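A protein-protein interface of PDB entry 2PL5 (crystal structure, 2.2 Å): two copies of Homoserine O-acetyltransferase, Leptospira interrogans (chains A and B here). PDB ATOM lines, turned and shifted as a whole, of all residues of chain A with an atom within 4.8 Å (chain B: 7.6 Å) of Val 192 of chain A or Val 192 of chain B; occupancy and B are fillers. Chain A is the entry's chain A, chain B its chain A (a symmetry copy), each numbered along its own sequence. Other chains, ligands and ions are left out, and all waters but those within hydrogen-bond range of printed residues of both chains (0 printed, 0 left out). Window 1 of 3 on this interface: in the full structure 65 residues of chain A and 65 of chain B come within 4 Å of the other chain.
OE1 of Glu 191 of chain A is in salt-bridge range of NH2 of Arg 194 of chain A (2.7 Å).
NE2 of Gln 195 of chain A is in hydrogen-bond range of OE2 of Glu 191 of chain A, at 3.0 Å.
The guanidinium group of Arg 194 of chain B lies within salt-bridge range of the side-chain carboxylate of Glu 191 of chain B.
OE2 of Glu 191 of chain B sits at hydrogen-bond distance from NE2 of Gln 195 of chain B (3.0 Å).
O of Ala 196 of chain B sits at hydrogen-bond distance from OG of Ser 199 of chain B, 3.4 Å away.
The backbone carbonyl oxygen (O) of Val 223 of chain B is in hydrogen-bond range of the side-chain hydroxyl (OG1) of Thr 227 of chain B, 2.8 Å away.
Among the printed residues, merely in contact across the chains: Ala 188 of chain A with Phe 189 of chain B (3.9 Å), Ala 188 of chain A with Ile 226 of chain B (3.7 Å), Phe 189 of chain A with Ala 188 of chain B (3.9 Å), Phe 189 of chain A with Phe 189 of chain B (3.5 Å), Glu 191 of chain A with Ile 226 of chain B (3.8 Å), Val 192 of chain A with Val 192 of chain B (3.7 Å), Val 192 of chain A with Leu 219 of chain B (3.97 Å), Val 192 of chain A with Met 222 of chain B (3.8 Å), Val 192 of chain A with Val 223 of chain B (3.9 Å), Val 192 of chain A with Ile 226 of chain B (3.8 Å), Gln 195 of chain A with Met 222 of chain B (3.3 Å), Ala 196 of chain A with Leu 219 of chain B (3.7 Å), Leu 219 of chain A with Val 192 of chain B (3.97 Å), Leu 219 of chain A with Ala 196 of chain B (3.7 Å), Leu 219 of chain A with Leu 219 of chain B (3.4 Å), Met 222 of chain A with Val 192 of chain B (3.8 Å), Met 222 of chain A with Gln 195 of chain B (3.3 Å), Val 223 of chain A with Val 192 of chain B (3.9 Å), Ile 226 of chain A with Ala 188 of chain B (3.7 Å), Ile 226 of chain A with Glu 191 of chain B (3.8 Å) and Ile 226 of chain A with Val 192 of chain B (3.8 Å).
Printed residues of chain B within 4 Å of Val 192 of chain A: Val 192 (3.7 Å), Leu 219 (3.97 Å), Met 222 (3.8 Å), Val 223 (3.9 Å) and Ile 226 (3.8 Å).
Val 192 of chain B touches five residues of chain A.
No residue of chain B comes within 4 Å of Gly 193 of chain A.
Of the printed residues of chain A, Ile 226 of chain B touches Ala 188, Glu 191 and Val 192.
Of the printed residues of chain A, Met 222 of chain B touches Val 192 and Gln 195.
Thr 227 of chain B touches none of the printed residues of chain A.
The nearest printed residue of chain A that does not touch Val 192 of chain B is Phe 189 of chain A (5.0 Å).
Printed residues of chain A that touch a printed residue of chain B: Ala 188, Phe 189, Glu 191, Val 192, Gln 195, Ala 196, Leu 219, Met 222, Val 223 and Ile 226.
Of the 25 printed residues of chain B, 10 touch a printed residue of chain A.
Among the printed residues, no Asp or Glu carboxylate lies within 4 Å of a Lys or Arg side-chain nitrogen of the other chain.
Val 192 of chain A touches its own counterpart, Val 192 of chain B.
Val 192 of chain A touches Val 223 of chain B, and with the chains exchanged Val 223 of chain A touches Val 192 of chain B.
Val 192 of chain A touches Ile 226 of chain B, and with the chains exchanged Ile 226 of chain A touches Val 192 of chain B.
Gln 195 of chain A touches Met 222 of chain B, and with the chains exchanged Met 222 of chain A touches Gln 195 of chain B.
13 positions are printed for both chains.
Of the 21 pairs that touch across the chains among the printed residues, 21 have their exchanged pair printed and touching as well.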
ATOM      1  N   ALA A 188       6.714  -2.960  15.814  1.00  0.00           N
ATOM      2  CA  ALA A 188       7.837  -2.473  16.629  1.00  0.00           C
ATOM      3  C   ALA A 188       8.275  -1.049  16.258  1.00  0.00           C
ATOM      4  O   ALA A 188       8.493  -0.223  17.145  1.00  0.00           O
ATOM      5  CB  ALA A 188       9.020  -3.444  16.558  1.00  0.00           C
ATOM      6  N   PHE A 189       8.406  -0.760  14.962  1.00  0.00           N
ATOM      7  CA  PHE A 189       8.729   0.601  14.526  1.00  0.00           C
ATOM      8  C   PHE A 189       7.676   1.613  14.984  1.00  0.00           C
ATOM      9  O   PHE A 189       8.023   2.714  15.419  1.00  0.00           O
ATOM     10  CB  PHE A 189       8.889   0.678  13.006  1.00  0.00           C
ATOM     11  CG  PHE A 189      10.240   0.218  12.501  1.00  0.00           C
ATOM     12  CD1 PHE A 189      10.336  -0.847  11.617  1.00  0.00           C
ATOM     13  CD2 PHE A 189      11.410   0.870  12.892  1.00  0.00           C
ATOM     14  CE1 PHE A 189      11.571  -1.269  11.146  1.00  0.00           C
ATOM     15  CE2 PHE A 189      12.651   0.450  12.424  1.00  0.00           C
ATOM     16  CZ  PHE A 189      12.727  -0.622  11.549  1.00  0.00           C
ATOM     17  N   ASN A 190       6.397   1.244  14.886  1.00  0.00           N
ATOM     18  CA  ASN A 190       5.302   2.126  15.324  1.00  0.00           C
ATOM     19  C   ASN A 190       5.259   2.291  16.832  1.00  0.00           C
ATOM     20  O   ASN A 190       5.026   3.388  17.338  1.00  0.00           O
ATOM     21  CB  ASN A 190       3.946   1.624  14.802  1.00  0.00           C
ATOM     22  CG  ASN A 190       3.829   1.738  13.292  1.00  0.00           C
ATOM     23  OD1 ASN A 190       4.470   2.588  12.679  1.00  0.00           O
ATOM     24  ND2 ASN A 190       2.994   0.891  12.686  1.00  0.00           N
ATOM     25  N   GLU A 191       5.491   1.191  17.541  1.00  0.00           N
ATOM     26  CA  GLU A 191       5.539   1.210  18.998  1.00  0.00           C
ATOM     27  C   GLU A 191       6.653   2.127  19.533  1.00  0.00           C
ATOM     28  O   GLU A 191       6.430   2.907  20.450  1.00  0.00           O
ATOM     29  CB  GLU A 191       5.677  -0.222  19.533  1.00  0.00           C
ATOM     30  CG  GLU A 191       5.380  -0.366  21.017  1.00  0.00           C
ATOM     31  CD  GLU A 191       3.946  -0.022  21.385  1.00  0.00           C
ATOM     32  OE1 GLU A 191       3.017  -0.380  20.633  1.00  0.00           O
ATOM     33  OE2 GLU A 191       3.746   0.605  22.445  1.00  0.00           O
ATOM     34  N   VAL A 192       7.842   2.041  18.943  1.00  0.00           N
ATOM     35  CA  VAL A 192       8.942   2.960  19.278  1.00  0.00           C
ATOM     36  C   VAL A 192       8.540   4.428  19.039  1.00  0.00           C
ATOM     37  O   VAL A 192       8.779   5.291  19.889  1.00  0.00           O
ATOM     38  CB  VAL A 192      10.244   2.608  18.501  1.00  0.00           C
ATOM     39  CG1 VAL A 192      11.332   3.641  18.767  1.00  0.00           C
ATOM     40  CG2 VAL A 192      10.740   1.238  18.908  1.00  0.00           C
ATOM     41  N   GLY A 193       7.913   4.699  17.891  1.00  0.00           N
ATOM     42  CA  GLY A 193       7.411   6.043  17.593  1.00  0.00           C
ATOM     43  C   GLY A 193       6.400   6.537  18.617  1.00  0.00           C
ATOM     44  O   GLY A 193       6.473   7.679  19.082  1.00  0.00           O
ATOM     45  N   ARG A 194       5.456   5.670  18.975  1.00  0.00           N
ATOM     46  CA  ARG A 194       4.419   6.004  19.951  1.00  0.00           C
ATOM     47  C   ARG A 194       5.018   6.272  21.342  1.00  0.00           C
ATOM     48  O   ARG A 194       4.591   7.182  22.047  1.00  0.00           O
ATOM     49  CB  ARG A 194       3.361   4.886  20.012  1.00  0.00           C
ATOM     50  CG  ARG A 194       2.428   4.808  18.772  1.00  0.00           C
ATOM     51  CD  ARG A 194       1.247   3.851  19.021  1.00  0.00           C
ATOM     52  NE  ARG A 194       1.675   2.455  19.086  1.00  0.00           N
ATOM     53  CZ  ARG A 194       1.569   1.577  18.089  1.00  0.00           C
ATOM     54  NH1 ARG A 194       1.005   1.918  16.935  1.00  0.00           N
ATOM     55  NH2 ARG A 194       2.005   0.341  18.254  1.00  0.00           N
ATOM     56  N   GLN A 195       6.015   5.479  21.724  1.00  0.00           N
ATOM     57  CA  GLN A 195       6.693   5.644  23.004  1.00  0.00           C
ATOM     58  C   GLN A 195       7.522   6.923  23.055  1.00  0.00           C
ATOM     59  O   GLN A 195       7.670   7.526  24.107  1.00  0.00           O
ATOM     60  CB  GLN A 195       7.575   4.425  23.304  1.00  0.00           C
ATOM     61  CG  GLN A 195       6.814   3.110  23.520  1.00  0.00           C
ATOM     62  CD  GLN A 195       5.827   3.166  24.669  1.00  0.00           C
ATOM     63  OE1 GLN A 195       5.898   4.049  25.528  1.00  0.00           O
ATOM     64  NE2 GLN A 195       4.895   2.216  24.692  1.00  0.00           N
ATOM     65  N   ALA A 196       8.069   7.321  21.902  1.00  0.00           N
ATOM     66  CA  ALA A 196       8.822   8.575  21.792  1.00  0.00           C
ATOM     67  C   ALA A 196       7.928   9.775  22.090  1.00  0.00           C
ATOM     68  O   ALA A 196       8.350  10.734  22.757  1.00  0.00           O
ATOM     69  CB  ALA A 196       9.457   8.712  20.406  1.00  0.00           C
ATOM     70  N   LEU A 219      10.944  12.204  16.222  1.00  0.00           N
ATOM     71  CA  LEU A 219      11.484  10.862  16.341  1.00  0.00           C
ATOM     72  C   LEU A 219      10.569   9.810  15.704  1.00  0.00           C
ATOM     73  O   LEU A 219      11.032   8.972  14.922  1.00  0.00           O
ATOM     74  CB  LEU A 219      11.744  10.542  17.814  1.00  0.00           C
ATOM     75  CG  LEU A 219      12.769   9.461  18.175  1.00  0.00           C
ATOM     76  CD1 LEU A 219      14.047   9.566  17.352  1.00  0.00           C
ATOM     77  CD2 LEU A 219      13.100   9.625  19.630  1.00  0.00           C
ATOM     78  N   MET A 222      10.780  10.228  11.914  1.00  0.00           N
ATOM     79  CA  MET A 222      12.124  10.002  11.394  1.00  0.00           C
ATOM     80  C   MET A 222      12.274   8.554  10.977  1.00  0.00           C
ATOM     81  O   MET A 222      12.970   8.238  10.007  1.00  0.00           O
ATOM     82  CB  MET A 222      13.150  10.338  12.465  1.00  0.00           C
ATOM     83  CG  MET A 222      14.573  10.199  12.005  1.00  0.00           C
ATOM     84  SD  MET A 222      15.662  10.056  13.413  1.00  0.00           S
ATOM     85  CE  MET A 222      14.981   8.588  14.191  1.00  0.00           C
ATOM     86  N   VAL A 223      11.601   7.686  11.727  1.00  0.00           N
ATOM     87  CA  VAL A 223      11.529   6.270  11.432  1.00  0.00           C
ATOM     88  C   VAL A 223      11.179   6.045   9.958  1.00  0.00           C
ATOM     89  O   VAL A 223      11.824   5.245   9.290  1.00  0.00           O
ATOM     90  CB  VAL A 223      10.516   5.544  12.367  1.00  0.00           C
ATOM     91  CG1 VAL A 223      10.538   4.055  12.115  1.00  0.00           C
ATOM     92  CG2 VAL A 223      10.817   5.832  13.839  1.00  0.00           C
ATOM     93  N   ILE A 226      14.318   7.103   7.824  1.00  0.00           N
ATOM     94  CA  ILE A 226      15.449   6.172   7.984  1.00  0.00           C
ATOM     95  C   ILE A 226      15.187   4.850   7.281  1.00  0.00           C
ATOM     96  O   ILE A 226      16.077   4.291   6.641  1.00  0.00           O
ATOM     97  CB  ILE A 226      15.750   5.871   9.471  1.00  0.00           C
ATOM     98  CG1 ILE A 226      16.120   7.149  10.218  1.00  0.00           C
ATOM     99  CG2 ILE A 226      16.885   4.843   9.605  1.00  0.00           C
ATOM    100  CD1 ILE A 226      16.186   6.970  11.718  1.00  0.00           C
ATOM    101  N   GLN B 186      17.830  -3.711  10.608  1.00  0.00           N
ATOM    102  CA  GLN B 186      18.662  -3.716  11.812  1.00  0.00           C
ATOM    103  C   GLN B 186      19.327  -2.366  12.074  1.00  0.00           C
ATOM    104  O   GLN B 186      19.332  -1.872  13.203  1.00  0.00           O
ATOM    105  CB  GLN B 186      19.723  -4.814  11.695  1.00  0.00           C
ATOM    106  CG  GLN B 186      19.160  -6.231  11.874  1.00  0.00           C
ATOM    107  CD  GLN B 186      20.061  -7.311  11.313  1.00  0.00           C
ATOM    108  OE1 GLN B 186      20.659  -7.157  10.248  1.00  0.00           O
ATOM    109  NE2 GLN B 186      20.128  -8.432  12.008  1.00  0.00           N
ATOM    110  N   ILE B 187      19.880  -1.777  11.022  1.00  0.00           N
ATOM    111  CA  ILE B 187      20.502  -0.462  11.097  1.00  0.00           C
ATOM    112  C   ILE B 187      19.476   0.616  11.465  1.00  0.00           C
ATOM    113  O   ILE B 187      19.776   1.505  12.256  1.00  0.00           O
ATOM    114  CB  ILE B 187      21.197  -0.107   9.760  1.00  0.00           C
ATOM    115  CG1 ILE B 187      22.345  -1.092   9.478  1.00  0.00           C
ATOM    116  CG2 ILE B 187      21.676   1.350   9.761  1.00  0.00           C
ATOM    117  CD1 ILE B 187      23.052  -0.867   8.144  1.00  0.00           C
ATOM    118  N   ALA B 188      18.272   0.517  10.901  1.00  0.00           N
ATOM    119  CA  ALA B 188      17.190   1.467  11.200  1.00  0.00           C
ATOM    120  C   ALA B 188      16.793   1.479  12.682  1.00  0.00           C
ATOM    121  O   ALA B 188      16.629   2.551  13.266  1.00  0.00           O
ATOM    122  CB  ALA B 188      15.972   1.199  10.310  1.00  0.00           C
ATOM    123  N   PHE B 189      16.637   0.301  13.290  1.00  0.00           N
ATOM    124  CA  PHE B 189      16.350   0.230  14.725  1.00  0.00           C
ATOM    125  C   PHE B 189      17.450   0.889  15.561  1.00  0.00           C
ATOM    126  O   PHE B 189      17.155   1.597  16.527  1.00  0.00           O
ATOM    127  CB  PHE B 189      16.151  -1.216  15.184  1.00  0.00           C
ATOM    128  CG  PHE B 189      14.771  -1.771  14.903  1.00  0.00           C
ATOM    129  CD1 PHE B 189      14.613  -2.889  14.096  1.00  0.00           C
ATOM    130  CD2 PHE B 189      13.636  -1.189  15.468  1.00  0.00           C
ATOM    131  CE1 PHE B 189      13.352  -3.406  13.840  1.00  0.00           C
ATOM    132  CE2 PHE B 189      12.369  -1.702  15.213  1.00  0.00           C
ATOM    133  CZ  PHE B 189      12.231  -2.814  14.397  1.00  0.00           C
ATOM    134  N   ASN B 190      18.712   0.657  15.193  1.00  0.00           N
ATOM    135  CA  ASN B 190      19.850   1.261  15.907  1.00  0.00           C
ATOM    136  C   ASN B 190      19.940   2.760  15.688  1.00  0.00           C
ATOM    137  O   ASN B 190      20.225   3.516  16.616  1.00  0.00           O
ATOM    138  CB  ASN B 190      21.173   0.583  15.515  1.00  0.00           C
ATOM    139  CG  ASN B 190      21.252  -0.854  16.000  1.00  0.00           C
ATOM    140  OD1 ASN B 190      20.625  -1.212  16.993  1.00  0.00           O
ATOM    141  ND2 ASN B 190      22.040  -1.682  15.309  1.00  0.00           N
ATOM    142  N   GLU B 191      19.689   3.180  14.452  1.00  0.00           N
ATOM    143  CA  GLU B 191      19.681   4.597  14.107  1.00  0.00           C
ATOM    144  C   GLU B 191      18.616   5.383  14.891  1.00  0.00           C
ATOM    145  O   GLU B 191      18.892   6.457  15.410  1.00  0.00           O
ATOM    146  CB  GLU B 191      19.507   4.763  12.591  1.00  0.00           C
ATOM    147  CG  GLU B 191      19.840   6.152  12.071  1.00  0.00           C
ATOM    148  CD  GLU B 191      21.295   6.543  12.274  1.00  0.00           C
ATOM    149  OE1 GLU B 191      22.190   5.693  12.090  1.00  0.00           O
ATOM    150  OE2 GLU B 191      21.546   7.718  12.610  1.00  0.00           O
ATOM    151  N   VAL B 192      17.409   4.833  14.988  1.00  0.00           N
ATOM    152  CA  VAL B 192      16.352   5.425  15.824  1.00  0.00           C
ATOM    153  C   VAL B 192      16.799   5.545  17.293  1.00  0.00           C
ATOM    154  O   VAL B 192      16.614   6.592  17.923  1.00  0.00           O
ATOM    155  CB  VAL B 192      15.018   4.632  15.713  1.00  0.00           C
ATOM    156  CG1 VAL B 192      13.974   5.185  16.677  1.00  0.00           C
ATOM    157  CG2 VAL B 192      14.484   4.701  14.300  1.00  0.00           C
ATOM    158  N   GLY B 193      17.404   4.480  17.825  1.00  0.00           N
ATOM    159  CA  GLY B 193      17.944   4.509  19.188  1.00  0.00           C
ATOM    160  C   GLY B 193      19.000   5.587  19.382  1.00  0.00           C
ATOM    161  O   GLY B 193      18.980   6.325  20.372  1.00  0.00           O
ATOM    162  N   ARG B 194      19.922   5.684  18.427  1.00  0.00           N
ATOM    163  CA  ARG B 194      20.997   6.675  18.477  1.00  0.00           C
ATOM    164  C   ARG B 194      20.446   8.109  18.405  1.00  0.00           C
ATOM    165  O   ARG B 194      20.924   9.003  19.097  1.00  0.00           O
ATOM    166  CB  ARG B 194      22.015   6.418  17.351  1.00  0.00           C
ATOM    167  CG  ARG B 194      22.911   5.166  17.560  1.00  0.00           C
ATOM    168  CD  ARG B 194      24.064   5.126  16.540  1.00  0.00           C
ATOM    169  NE  ARG B 194      23.589   4.855  15.184  1.00  0.00           N
ATOM    170  CZ  ARG B 194      23.636   3.668  14.581  1.00  0.00           C
ATOM    171  NH1 ARG B 194      24.179   2.617  15.184  1.00  0.00           N
ATOM    172  NH2 ARG B 194      23.161   3.535  13.355  1.00  0.00           N
ATOM    173  N   GLN B 195      19.433   8.317  17.569  1.00  0.00           N
ATOM    174  CA  GLN B 195      18.796   9.620  17.427  1.00  0.00           C
ATOM    175  C   GLN B 195      18.015  10.018  18.675  1.00  0.00           C
ATOM    176  O   GLN B 195      17.918  11.192  18.999  1.00  0.00           O
ATOM    177  CB  GLN B 195      17.880   9.638  16.197  1.00  0.00           C
ATOM    178  CG  GLN B 195      18.599   9.492  14.849  1.00  0.00           C
ATOM    179  CD  GLN B 195      19.619  10.583  14.588  1.00  0.00           C
ATOM    180  OE1 GLN B 195      19.603  11.637  15.230  1.00  0.00           O
ATOM    181  NE2 GLN B 195      20.517  10.336  13.637  1.00  0.00           N
ATOM    182  N   ALA B 196      17.451   9.021  19.363  1.00  0.00           N
ATOM    183  CA  ALA B 196      16.740   9.254  20.625  1.00  0.00           C
ATOM    184  C   ALA B 196      17.683   9.810  21.688  1.00  0.00           C
ATOM    185  O   ALA B 196      17.314  10.710  22.460  1.00  0.00           O
ATOM    186  CB  ALA B 196      16.072   7.970  21.123  1.00  0.00           C
ATOM    187  N   ILE B 197      18.908   9.279  21.713  1.00  0.00           N
ATOM    188  CA  ILE B 197      19.951   9.757  22.620  1.00  0.00           C
ATOM    189  C   ILE B 197      20.427  11.149  22.192  1.00  0.00           C
ATOM    190  O   ILE B 197      20.550  12.058  23.030  1.00  0.00           O
ATOM    191  CB  ILE B 197      21.154   8.773  22.669  1.00  0.00           C
ATOM    192  CG1 ILE B 197      20.747   7.454  23.347  1.00  0.00           C
ATOM    193  CG2 ILE B 197      22.334   9.407  23.389  1.00  0.00           C
ATOM    194  CD1 ILE B 197      21.600   6.246  22.975  1.00  0.00           C
ATOM    195  N   LEU B 198      20.692  11.311  20.893  1.00  0.00           N
ATOM    196  CA  LEU B 198      21.205  12.576  20.354  1.00  0.00           C
ATOM    197  C   LEU B 198      20.270  13.756  20.591  1.00  0.00           C
ATOM    198  O   LEU B 198      20.738  14.872  20.812  1.00  0.00           O
ATOM    199  CB  LEU B 198      21.539  12.469  18.861  1.00  0.00           C
ATOM    200  CG  LEU B 198      22.680  11.529  18.443  1.00  0.00           C
ATOM    201  CD1 LEU B 198      22.882  11.564  16.925  1.00  0.00           C
ATOM    202  CD2 LEU B 198      23.983  11.858  19.158  1.00  0.00           C
ATOM    203  N   SER B 199      18.961  13.500  20.561  1.00  0.00           N
ATOM    204  CA  SER B 199      17.935  14.531  20.718  1.00  0.00           C
ATOM    205  C   SER B 199      17.480  14.721  22.165  1.00  0.00           C
ATOM    206  O   SER B 199      16.671  15.597  22.459  1.00  0.00           O
ATOM    207  CB  SER B 199      16.725  14.218  19.827  1.00  0.00           C
ATOM    208  OG  SER B 199      16.086  13.008  20.208  1.00  0.00           O
ATOM    209  N   GLY B 216      16.492   9.235  26.540  1.00  0.00           N
ATOM    210  CA  GLY B 216      16.935   8.824  25.208  1.00  0.00           C
ATOM    211  C   GLY B 216      17.414   7.389  25.167  1.00  0.00           C
ATOM    212  O   GLY B 216      17.055   6.628  24.265  1.00  0.00           O
ATOM    213  N   LEU B 219      14.595   4.844  25.590  1.00  0.00           N
ATOM    214  CA  LEU B 219      14.012   4.644  24.277  1.00  0.00           C
ATOM    215  C   LEU B 219      14.871   3.733  23.392  1.00  0.00           C
ATOM    216  O   LEU B 219      14.358   2.783  22.790  1.00  0.00           O
ATOM    217  CB  LEU B 219      13.781   5.998  23.605  1.00  0.00           C
ATOM    218  CG  LEU B 219      12.729   6.114  22.497  1.00  0.00           C
ATOM    219  CD1 LEU B 219      11.433   5.390  22.840  1.00  0.00           C
ATOM    220  CD2 LEU B 219      12.444   7.575  22.300  1.00  0.00           C
ATOM    221  N   ALA B 220      16.172   4.019  23.327  1.00  0.00           N
ATOM    222  CA  ALA B 220      17.117   3.221  22.541  1.00  0.00           C
ATOM    223  C   ALA B 220      17.076   1.741  22.913  1.00  0.00           C
ATOM    224  O   ALA B 220      17.138   0.878  22.041  1.00  0.00           O
ATOM    225  CB  ALA B 220      18.529   3.761  22.694  1.00  0.00           C
ATOM    226  N   MET B 222      14.571   0.176  24.752  1.00  0.00           N
ATOM    227  CA  MET B 222      13.206  -0.336  24.701  1.00  0.00           C
ATOM    228  C   MET B 222      12.994  -1.095  23.407  1.00  0.00           C
ATOM    229  O   MET B 222      12.260  -2.088  23.364  1.00  0.00           O
ATOM    230  CB  MET B 222      12.223   0.821  24.786  1.00  0.00           C
ATOM    231  CG  MET B 222      10.783   0.392  24.805  1.00  0.00           C
ATOM    232  SD  MET B 222       9.729   1.757  24.345  1.00  0.00           S
ATOM    233  CE  MET B 222      10.379   2.120  22.710  1.00  0.00           C
ATOM    234  N   VAL B 223      13.656  -0.610  22.361  1.00  0.00           N
ATOM    235  CA  VAL B 223      13.669  -1.251  21.063  1.00  0.00           C
ATOM    236  C   VAL B 223      13.970  -2.746  21.205  1.00  0.00           C
ATOM    237  O   VAL B 223      13.279  -3.569  20.615  1.00  0.00           O
ATOM    238  CB  VAL B 223      14.681  -0.563  20.098  1.00  0.00           C
ATOM    239  CG1 VAL B 223      14.599  -1.177  18.721  1.00  0.00           C
ATOM    240  CG2 VAL B 223      14.431   0.944  20.017  1.00  0.00           C
ATOM    241  N   GLY B 224      14.977  -3.092  22.007  1.00  0.00           N
ATOM    242  CA  GLY B 224      15.333  -4.492  22.246  1.00  0.00           C
ATOM    243  C   GLY B 224      14.286  -5.291  23.004  1.00  0.00           C
ATOM    244  O   GLY B 224      14.207  -6.508  22.856  1.00  0.00           O
ATOM    245  N   ILE B 226      10.813  -4.436  22.849  1.00  0.00           N
ATOM    246  CA  ILE B 226       9.655  -4.473  21.939  1.00  0.00           C
ATOM    247  C   ILE B 226       9.851  -5.492  20.828  1.00  0.00           C
ATOM    248  O   ILE B 226       8.924  -6.220  20.472  1.00  0.00           O
ATOM    249  CB  ILE B 226       9.385  -3.098  21.284  1.00  0.00           C
ATOM    250  CG1 ILE B 226       9.081  -2.044  22.344  1.00  0.00           C
ATOM    251  CG2 ILE B 226       8.217  -3.185  20.286  1.00  0.00           C
ATOM    252  CD1 ILE B 226       9.050  -0.635  21.796  1.00  0.00           C
ATOM    253  N   THR B 227      11.060  -5.536  20.282  1.00  0.00           N
ATOM    254  CA  THR B 227      11.402  -6.481  19.223  1.00  0.00           C
ATOM    255  C   THR B 227      11.493  -7.942  19.702  1.00  0.00           C
ATOM    256  O   THR B 227      11.702  -8.844  18.889  1.00  0.00           O
ATOM    257  CB  THR B 227      12.727  -6.083  18.505  1.00  0.00           C
ATOM    258  OG1 THR B 227      13.787  -6.024  19.458  1.00  0.00           O
ATOM    259  CG2 THR B 227      12.601  -4.715  17.822  1.00  0.00           C
ATOM    260  N   ILE B 259       8.628   3.175  28.872  1.00  0.00           N
ATOM    261  CA  ILE B 259       9.883   3.340  28.126  1.00  0.00           C
ATOM    262  C   ILE B 259      11.032   2.507  28.730  1.00  0.00           C
ATOM    263  O   ILE B 259      11.959   2.107  28.024  1.00  0.00           O
ATOM    264  CB  ILE B 259      10.274   4.853  28.004  1.00  0.00           C
ATOM    265  CG1 ILE B 259      11.301   5.078  26.884  1.00  0.00           C
ATOM    266  CG2 ILE B 259      10.735   5.434  29.360  1.00  0.00           C
ATOM    267  CD1 ILE B 259      11.779   6.524  26.756  1.00  0.00           C
ATOM    268  N   TYR B 274      26.251   2.750  23.957  1.00  0.00           N
ATOM    269  CA  TYR B 274      25.237   2.312  22.997  1.00  0.00           C
ATOM    270  C   TYR B 274      25.536   2.827  21.594  1.00  0.00           C
ATOM    271  O   TYR B 274      25.465   2.079  20.626  1.00  0.00           O
ATOM    272  CB  TYR B 274      23.834   2.760  23.434  1.00  0.00           C
ATOM    273  CG  TYR B 274      22.759   2.403  22.425  1.00  0.00           C
ATOM    274  CD1 TYR B 274      22.025   1.222  22.537  1.00  0.00           C
ATOM    275  CD2 TYR B 274      22.495   3.240  21.338  1.00  0.00           C
ATOM    276  CE1 TYR B 274      21.035   0.891  21.589  1.00  0.00           C
ATOM    277  CE2 TYR B 274      21.512   2.923  20.401  1.00  0.00           C
ATOM    278  CZ  TYR B 274      20.790   1.755  20.531  1.00  0.00           C
ATOM    279  OH  TYR B 274      19.823   1.467  19.586  1.00  0.00           O
ATOM    280  N   ASP B 282      26.672  -1.817  12.952  1.00  0.00           N
ATOM    281  CA  ASP B 282      26.103  -1.305  11.707  1.00  0.00           C
ATOM    282  C   ASP B 282      27.115  -1.117  10.572  1.00  0.00           C
ATOM    283  O   ASP B 282      26.774  -1.285   9.396  1.00  0.00           O
ATOM    284  CB  ASP B 282      25.354   0.003  11.969  1.00  0.00           C
ATOM    285  CG  ASP B 282      24.062  -0.209  12.744  1.00  0.00           C
ATOM    286  OD1 ASP B 282      23.575  -1.360  12.812  1.00  0.00           O
ATOM    287  OD2 ASP B 282      23.533   0.783  13.273  1.00  0.00           O
